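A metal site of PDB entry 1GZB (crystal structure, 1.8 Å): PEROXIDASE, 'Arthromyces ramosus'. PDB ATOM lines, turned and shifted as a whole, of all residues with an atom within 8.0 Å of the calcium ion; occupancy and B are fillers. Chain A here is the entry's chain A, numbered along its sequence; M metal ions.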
ATOM      1  N   PRO A 130     -12.064   8.416 -11.139  1.00  0.00           N
ATOM      2  CA  PRO A 130     -12.521   8.217  -9.788  1.00  0.00           C
ATOM      3  C   PRO A 130     -12.290   6.821  -9.257  1.00  0.00           C
ATOM      4  O   PRO A 130     -12.480   5.835  -9.974  1.00  0.00           O
ATOM      5  CB  PRO A 130     -13.977   8.518  -9.819  1.00  0.00           C
ATOM      6  CG  PRO A 130     -14.158   9.433 -10.998  1.00  0.00           C
ATOM      7  CD  PRO A 130     -13.154   8.879 -11.999  1.00  0.00           C
ATOM      8  N   ALA A 182      -7.452  -5.722 -12.910  1.00  0.00           N
ATOM      9  CA  ALA A 182      -8.359  -4.708 -12.406  1.00  0.00           C
ATOM     10  C   ALA A 182      -8.389  -3.545 -13.438  1.00  0.00           C
ATOM     11  O   ALA A 182      -9.348  -2.758 -13.533  1.00  0.00           O
ATOM     12  CB  ALA A 182      -7.882  -4.127 -11.073  1.00  0.00           C
ATOM     13  N   ALA A 183      -7.366  -3.382 -14.274  1.00  0.00           N
ATOM     14  CA  ALA A 183      -7.370  -2.358 -15.273  1.00  0.00           C
ATOM     15  C   ALA A 183      -8.489  -2.617 -16.296  1.00  0.00           C
ATOM     16  O   ALA A 183      -8.892  -1.695 -17.013  1.00  0.00           O
ATOM     17  CB  ALA A 183      -6.012  -2.348 -15.930  1.00  0.00           C
ATOM     18  N   HIS A 184      -9.100  -3.809 -16.390  1.00  0.00           N
ATOM     19  CA  HIS A 184     -10.219  -3.965 -17.314  1.00  0.00           C
ATOM     20  C   HIS A 184     -11.519  -3.309 -16.763  1.00  0.00           C
ATOM     21  O   HIS A 184     -12.592  -3.299 -17.386  1.00  0.00           O
ATOM     22  CB  HIS A 184     -10.425  -5.440 -17.610  1.00  0.00           C
ATOM     23  CG  HIS A 184      -9.521  -5.986 -18.724  1.00  0.00           C
ATOM     24  ND1 HIS A 184      -9.688  -7.237 -19.314  1.00  0.00           N
ATOM     25  CD2 HIS A 184      -8.434  -5.340 -19.329  1.00  0.00           C
ATOM     26  CE1 HIS A 184      -8.762  -7.336 -20.283  1.00  0.00           C
ATOM     27  NE2 HIS A 184      -8.041  -6.273 -20.306  1.00  0.00           N
ATOM     28  N   SER A 185     -11.393  -2.647 -15.577  1.00  0.00           N
ATOM     29  CA  SER A 185     -12.498  -1.895 -14.991  1.00  0.00           C
ATOM     30  C   SER A 185     -12.554  -0.547 -15.691  1.00  0.00           C
ATOM     31  O   SER A 185     -13.554   0.132 -15.515  1.00  0.00           O
ATOM     32  CB  SER A 185     -12.258  -1.644 -13.527  1.00  0.00           C
ATOM     33  OG  SER A 185     -13.391  -1.200 -12.843  1.00  0.00           O
ATOM     34  N   LEU A 186     -11.554  -0.132 -16.482  1.00  0.00           N
ATOM     35  CA  LEU A 186     -11.501   1.162 -17.148  1.00  0.00           C
ATOM     36  C   LEU A 186     -11.246   0.766 -18.601  1.00  0.00           C
ATOM     37  O   LEU A 186     -10.246   1.145 -19.212  1.00  0.00           O
ATOM     38  CB  LEU A 186     -10.322   1.903 -16.501  1.00  0.00           C
ATOM     39  CG  LEU A 186     -10.364   3.018 -15.443  1.00  0.00           C
ATOM     40  CD1 LEU A 186     -11.755   3.192 -14.861  1.00  0.00           C
ATOM     41  CD2 LEU A 186      -9.235   2.745 -14.468  1.00  0.00           C
ATOM     42  N   ALA A 187     -12.164   0.034 -19.201  1.00  0.00           N
ATOM     43  CA  ALA A 187     -11.892  -0.537 -20.498  1.00  0.00           C
ATOM     44  C   ALA A 187     -12.988  -0.764 -21.489  1.00  0.00           C
ATOM     45  O   ALA A 187     -14.138  -0.925 -21.106  1.00  0.00           O
ATOM     46  CB  ALA A 187     -11.227  -1.883 -20.262  1.00  0.00           C
ATOM     47  N   LEU A 201     -16.153  -3.008 -21.018  1.00  0.00           N
ATOM     48  CA  LEU A 201     -15.940  -4.329 -20.449  1.00  0.00           C
ATOM     49  C   LEU A 201     -16.617  -4.413 -19.080  1.00  0.00           C
ATOM     50  O   LEU A 201     -16.750  -5.503 -18.517  1.00  0.00           O
ATOM     51  CB  LEU A 201     -14.445  -4.583 -20.381  1.00  0.00           C
ATOM     52  CG  LEU A 201     -13.787  -5.334 -21.542  1.00  0.00           C
ATOM     53  CD1 LEU A 201     -14.358  -4.997 -22.902  1.00  0.00           C
ATOM     54  CD2 LEU A 201     -12.304  -5.091 -21.397  1.00  0.00           C
ATOM     55  N   ASP A 202     -17.069  -3.317 -18.488  1.00  0.00           N
ATOM     56  CA  ASP A 202     -17.866  -3.391 -17.294  1.00  0.00           C
ATOM     57  C   ASP A 202     -18.810  -2.184 -17.372  1.00  0.00           C
ATOM     58  O   ASP A 202     -18.594  -1.304 -18.190  1.00  0.00           O
ATOM     59  CB  ASP A 202     -16.991  -3.363 -16.025  1.00  0.00           C
ATOM     60  CG  ASP A 202     -16.335  -2.094 -15.474  1.00  0.00           C
ATOM     61  OD1 ASP A 202     -16.396  -0.993 -16.029  1.00  0.00           O
ATOM     62  OD2 ASP A 202     -15.770  -2.229 -14.400  1.00  0.00           O
ATOM     63  N   SER A 203     -19.826  -2.055 -16.532  1.00  0.00           N
ATOM     64  CA  SER A 203     -20.778  -0.953 -16.630  1.00  0.00           C
ATOM     65  C   SER A 203     -20.276   0.426 -16.228  1.00  0.00           C
ATOM     66  O   SER A 203     -21.028   1.388 -16.327  1.00  0.00           O
ATOM     67  CB  SER A 203     -22.008  -1.267 -15.784  1.00  0.00           C
ATOM     68  OG  SER A 203     -21.632  -1.548 -14.430  1.00  0.00           O
ATOM     69  N   THR A 204     -19.070   0.538 -15.675  1.00  0.00           N
ATOM     70  CA  THR A 204     -18.544   1.819 -15.275  1.00  0.00           C
ATOM     71  C   THR A 204     -17.154   2.006 -15.902  1.00  0.00           C
ATOM     72  O   THR A 204     -16.187   2.055 -15.141  1.00  0.00           O
ATOM     73  CB  THR A 204     -18.466   1.866 -13.757  1.00  0.00           C
ATOM     74  OG1 THR A 204     -17.728   0.699 -13.362  1.00  0.00           O
ATOM     75  CG2 THR A 204     -19.825   1.885 -13.086  1.00  0.00           C
ATOM     76  N   PRO A 205     -16.980   2.173 -17.231  1.00  0.00           N
ATOM     77  CA  PRO A 205     -15.666   2.310 -17.860  1.00  0.00           C
ATOM     78  C   PRO A 205     -14.918   3.542 -17.401  1.00  0.00           C
ATOM     79  O   PRO A 205     -13.775   3.720 -17.854  1.00  0.00           O
ATOM     80  CB  PRO A 205     -15.933   2.331 -19.379  1.00  0.00           C
ATOM     81  CG  PRO A 205     -17.297   3.007 -19.469  1.00  0.00           C
ATOM     82  CD  PRO A 205     -18.021   2.311 -18.268  1.00  0.00           C
ATOM     83  N   GLN A 206     -15.543   4.444 -16.646  1.00  0.00           N
ATOM     84  CA  GLN A 206     -14.828   5.606 -16.189  1.00  0.00           C
ATOM     85  C   GLN A 206     -14.638   5.574 -14.694  1.00  0.00           C
ATOM     86  O   GLN A 206     -14.227   6.581 -14.140  1.00  0.00           O
ATOM     87  CB  GLN A 206     -15.575   6.879 -16.598  1.00  0.00           C
ATOM     88  CG  GLN A 206     -15.328   7.283 -18.032  1.00  0.00           C
ATOM     89  CD  GLN A 206     -15.952   8.618 -18.396  1.00  0.00           C
ATOM     90  OE1 GLN A 206     -17.152   8.798 -18.229  1.00  0.00           O
ATOM     91  NE2 GLN A 206     -15.253   9.623 -18.887  1.00  0.00           N
ATOM     92  N   VAL A 207     -14.893   4.457 -13.991  1.00  0.00           N
ATOM     93  CA  VAL A 207     -14.743   4.401 -12.541  1.00  0.00           C
ATOM     94  C   VAL A 207     -13.849   3.198 -12.262  1.00  0.00           C
ATOM     95  O   VAL A 207     -14.152   2.104 -12.739  1.00  0.00           O
ATOM     96  CB  VAL A 207     -16.098   4.200 -11.798  1.00  0.00           C
ATOM     97  CG1 VAL A 207     -15.870   4.278 -10.295  1.00  0.00           C
ATOM     98  CG2 VAL A 207     -17.095   5.240 -12.231  1.00  0.00           C
ATOM     99  N   PHE A 208     -12.753   3.346 -11.513  1.00  0.00           N
ATOM    100  CA  PHE A 208     -11.872   2.235 -11.183  1.00  0.00           C
ATOM    101  C   PHE A 208     -12.577   1.588  -9.992  1.00  0.00           C
ATOM    102  O   PHE A 208     -12.538   2.110  -8.857  1.00  0.00           O
ATOM    103  CB  PHE A 208     -10.494   2.740 -10.766  1.00  0.00           C
ATOM    104  CG  PHE A 208      -9.528   1.607 -10.462  1.00  0.00           C
ATOM    105  CD1 PHE A 208      -9.108   0.773 -11.465  1.00  0.00           C
ATOM    106  CD2 PHE A 208      -9.107   1.422  -9.166  1.00  0.00           C
ATOM    107  CE1 PHE A 208      -8.241  -0.249 -11.162  1.00  0.00           C
ATOM    108  CE2 PHE A 208      -8.252   0.395  -8.890  1.00  0.00           C
ATOM    109  CZ  PHE A 208      -7.825  -0.427  -9.887  1.00  0.00           C
ATOM    110  N   ASP A 209     -13.304   0.503 -10.291  1.00  0.00           N
ATOM    111  CA  ASP A 209     -14.051  -0.184  -9.280  1.00  0.00           C
ATOM    112  C   ASP A 209     -14.120  -1.709  -9.497  1.00  0.00           C
ATOM    113  O   ASP A 209     -13.602  -2.305 -10.437  1.00  0.00           O
ATOM    114  CB  ASP A 209     -15.488   0.440  -9.208  1.00  0.00           C
ATOM    115  CG  ASP A 209     -16.314   0.303 -10.491  1.00  0.00           C
ATOM    116  OD1 ASP A 209     -15.930  -0.410 -11.432  1.00  0.00           O
ATOM    117  OD2 ASP A 209     -17.359   0.924 -10.572  1.00  0.00           O
ATOM    118  N   THR A 210     -14.831  -2.348  -8.613  1.00  0.00           N
ATOM    119  CA  THR A 210     -15.032  -3.765  -8.553  1.00  0.00           C
ATOM    120  C   THR A 210     -15.976  -4.355  -9.608  1.00  0.00           C
ATOM    121  O   THR A 210     -16.005  -5.582  -9.804  1.00  0.00           O
ATOM    122  CB  THR A 210     -15.438  -3.839  -7.068  1.00  0.00           C
ATOM    123  OG1 THR A 210     -14.454  -4.582  -6.383  1.00  0.00           O
ATOM    124  CG2 THR A 210     -16.837  -4.305  -6.917  1.00  0.00           C
ATOM    125  N   GLN A 211     -16.763  -3.548 -10.337  1.00  0.00           N
ATOM    126  CA  GLN A 211     -17.757  -4.060 -11.256  1.00  0.00           C
ATOM    127  C   GLN A 211     -17.291  -5.032 -12.316  1.00  0.00           C
ATOM    128  O   GLN A 211     -18.040  -5.944 -12.662  1.00  0.00           O
ATOM    129  CB  GLN A 211     -18.456  -2.940 -11.979  1.00  0.00           C
ATOM    130  CG  GLN A 211     -19.279  -2.076 -11.094  1.00  0.00           C
ATOM    131  CD  GLN A 211     -20.301  -2.825 -10.248  1.00  0.00           C
ATOM    132  OE1 GLN A 211     -20.417  -2.607  -9.023  1.00  0.00           O
ATOM    133  NE2 GLN A 211     -21.061  -3.719 -10.829  1.00  0.00           N
ATOM    134  N   PHE A 212     -16.088  -4.874 -12.871  1.00  0.00           N
ATOM    135  CA  PHE A 212     -15.547  -5.793 -13.863  1.00  0.00           C
ATOM    136  C   PHE A 212     -15.550  -7.235 -13.325  1.00  0.00           C
ATOM    137  O   PHE A 212     -16.038  -8.145 -13.997  1.00  0.00           O
ATOM    138  CB  PHE A 212     -14.141  -5.341 -14.229  1.00  0.00           C
ATOM    139  CG  PHE A 212     -13.394  -6.389 -15.002  1.00  0.00           C
ATOM    140  CD1 PHE A 212     -13.725  -6.637 -16.316  1.00  0.00           C
ATOM    141  CD2 PHE A 212     -12.422  -7.119 -14.358  1.00  0.00           C
ATOM    142  CE1 PHE A 212     -13.070  -7.648 -16.996  1.00  0.00           C
ATOM    143  CE2 PHE A 212     -11.772  -8.123 -15.045  1.00  0.00           C
ATOM    144  CZ  PHE A 212     -12.099  -8.402 -16.360  1.00  0.00           C
ATOM    145  N   TYR A 213     -15.072  -7.444 -12.102  1.00  0.00           N
ATOM    146  CA  TYR A 213     -15.015  -8.754 -11.488  1.00  0.00           C
ATOM    147  C   TYR A 213     -16.395  -9.345 -11.319  1.00  0.00           C
ATOM    148  O   TYR A 213     -16.620 -10.485 -11.722  1.00  0.00           O
ATOM    149  CB  TYR A 213     -14.328  -8.644 -10.177  1.00  0.00           C
ATOM    150  CG  TYR A 213     -12.856  -8.305 -10.388  1.00  0.00           C
ATOM    151  CD1 TYR A 213     -12.006  -9.285 -10.869  1.00  0.00           C
ATOM    152  CD2 TYR A 213     -12.354  -7.035 -10.107  1.00  0.00           C
ATOM    153  CE1 TYR A 213     -10.649  -9.024 -11.055  1.00  0.00           C
ATOM    154  CE2 TYR A 213     -10.991  -6.788 -10.293  1.00  0.00           C
ATOM    155  CZ  TYR A 213     -10.157  -7.776 -10.757  1.00  0.00           C
ATOM    156  OH  TYR A 213      -8.800  -7.549 -10.900  1.00  0.00           O
ATOM    157  N   GLU A 215     -19.224  -8.538 -12.968  1.00  0.00           N
ATOM    158  CA  GLU A 215     -19.915  -8.715 -14.221  1.00  0.00           C
ATOM    159  C   GLU A 215     -19.384  -9.749 -15.197  1.00  0.00           C
ATOM    160  O   GLU A 215     -20.144 -10.154 -16.081  1.00  0.00           O
ATOM    161  CB  GLU A 215     -20.019  -7.376 -14.900  1.00  0.00           C
ATOM    162  CG  GLU A 215     -20.829  -6.403 -14.038  1.00  0.00           C
ATOM    163  CD  GLU A 215     -20.921  -4.970 -14.497  1.00  0.00           C
ATOM    164  OE1 GLU A 215     -20.637  -4.623 -15.644  1.00  0.00           O
ATOM    165  OE2 GLU A 215     -21.276  -4.166 -13.669  1.00  0.00           O
ATOM    166  N   ASN A 266     -13.491  -2.261  -2.995  1.00  0.00           N
ATOM    167  CA  ASN A 266     -12.712  -1.435  -3.876  1.00  0.00           C
ATOM    168  C   ASN A 266     -11.400  -1.097  -3.168  1.00  0.00           C
ATOM    169  O   ASN A 266     -10.396  -0.830  -3.816  1.00  0.00           O
ATOM    170  CB  ASN A 266     -13.461  -0.170  -4.184  1.00  0.00           C
ATOM    171  CG  ASN A 266     -14.639  -0.264  -5.149  1.00  0.00           C
ATOM    172  OD1 ASN A 266     -14.555  -0.771  -6.239  1.00  0.00           O
ATOM    173  ND2 ASN A 266     -15.776   0.299  -4.773  1.00  0.00           N
ATOM    174  N   MET A 269      -9.066  -4.297  -3.697  1.00  0.00           N
ATOM    175  CA  MET A 269      -8.736  -4.342  -5.099  1.00  0.00           C
ATOM    176  C   MET A 269      -7.686  -3.276  -5.443  1.00  0.00           C
ATOM    177  O   MET A 269      -6.685  -3.572  -6.101  1.00  0.00           O
ATOM    178  CB  MET A 269     -10.010  -4.109  -5.901  1.00  0.00           C
ATOM    179  CG  MET A 269      -9.683  -4.086  -7.403  1.00  0.00           C
ATOM    180  SD  MET A 269     -11.003  -3.520  -8.493  1.00  0.00           S
ATOM    181  CE  MET A 269     -10.829  -1.800  -8.229  1.00  0.00           C
ATOM    182  N   ASN A 303     -14.313   7.341  -5.048  1.00  0.00           N
ATOM    183  CA  ASN A 303     -15.511   6.718  -5.600  1.00  0.00           C
ATOM    184  C   ASN A 303     -16.357   6.408  -4.361  1.00  0.00           C
ATOM    185  O   ASN A 303     -15.849   5.703  -3.454  1.00  0.00           O
ATOM    186  CB  ASN A 303     -15.151   5.437  -6.269  1.00  0.00           C
ATOM    187  CG  ASN A 303     -16.366   4.569  -6.531  1.00  0.00           C
ATOM    188  OD1 ASN A 303     -17.478   5.050  -6.751  1.00  0.00           O
ATOM    189  ND2 ASN A 303     -16.159   3.253  -6.562  1.00  0.00           N
HETATM  190 CA    CA M   1     -15.352   0.216 -13.798  1.00  0.00          CA
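O of Thr 204 binds the calcium ion (2.4 Å). OG1 of Thr 204 binds the calcium ion (2.5 Å). O of Val 207 binds the calcium ion, 2.5 Å away. The calcium ion is bound by the backbone carbonyl oxygen (O) of Ser 185 (2.5 Å). OD1 of Asp 209 is bound to the calcium ion, at 2.5 Å. The side-chain carboxylate (OD2) of Asp 202 binds the calcium ion (2.6 Å). OG of Ser 185 binds the calcium ion (2.6 Å). The calcium ion is bound by OD1 of Asp 202, 2.7 Å away. The calcium ion has eight donor atoms within binding distance.
Of the 24 residues printed, 5 come within 4 Å of the calcium ion. Along chain A the residues within 4 Å of the calcium ion span positions 185 to 209.
N of Gln 211 sits close to OD1 of Asp 209. N of Phe 212 lies close to OD2 of Asp 202 (3.1 Å).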
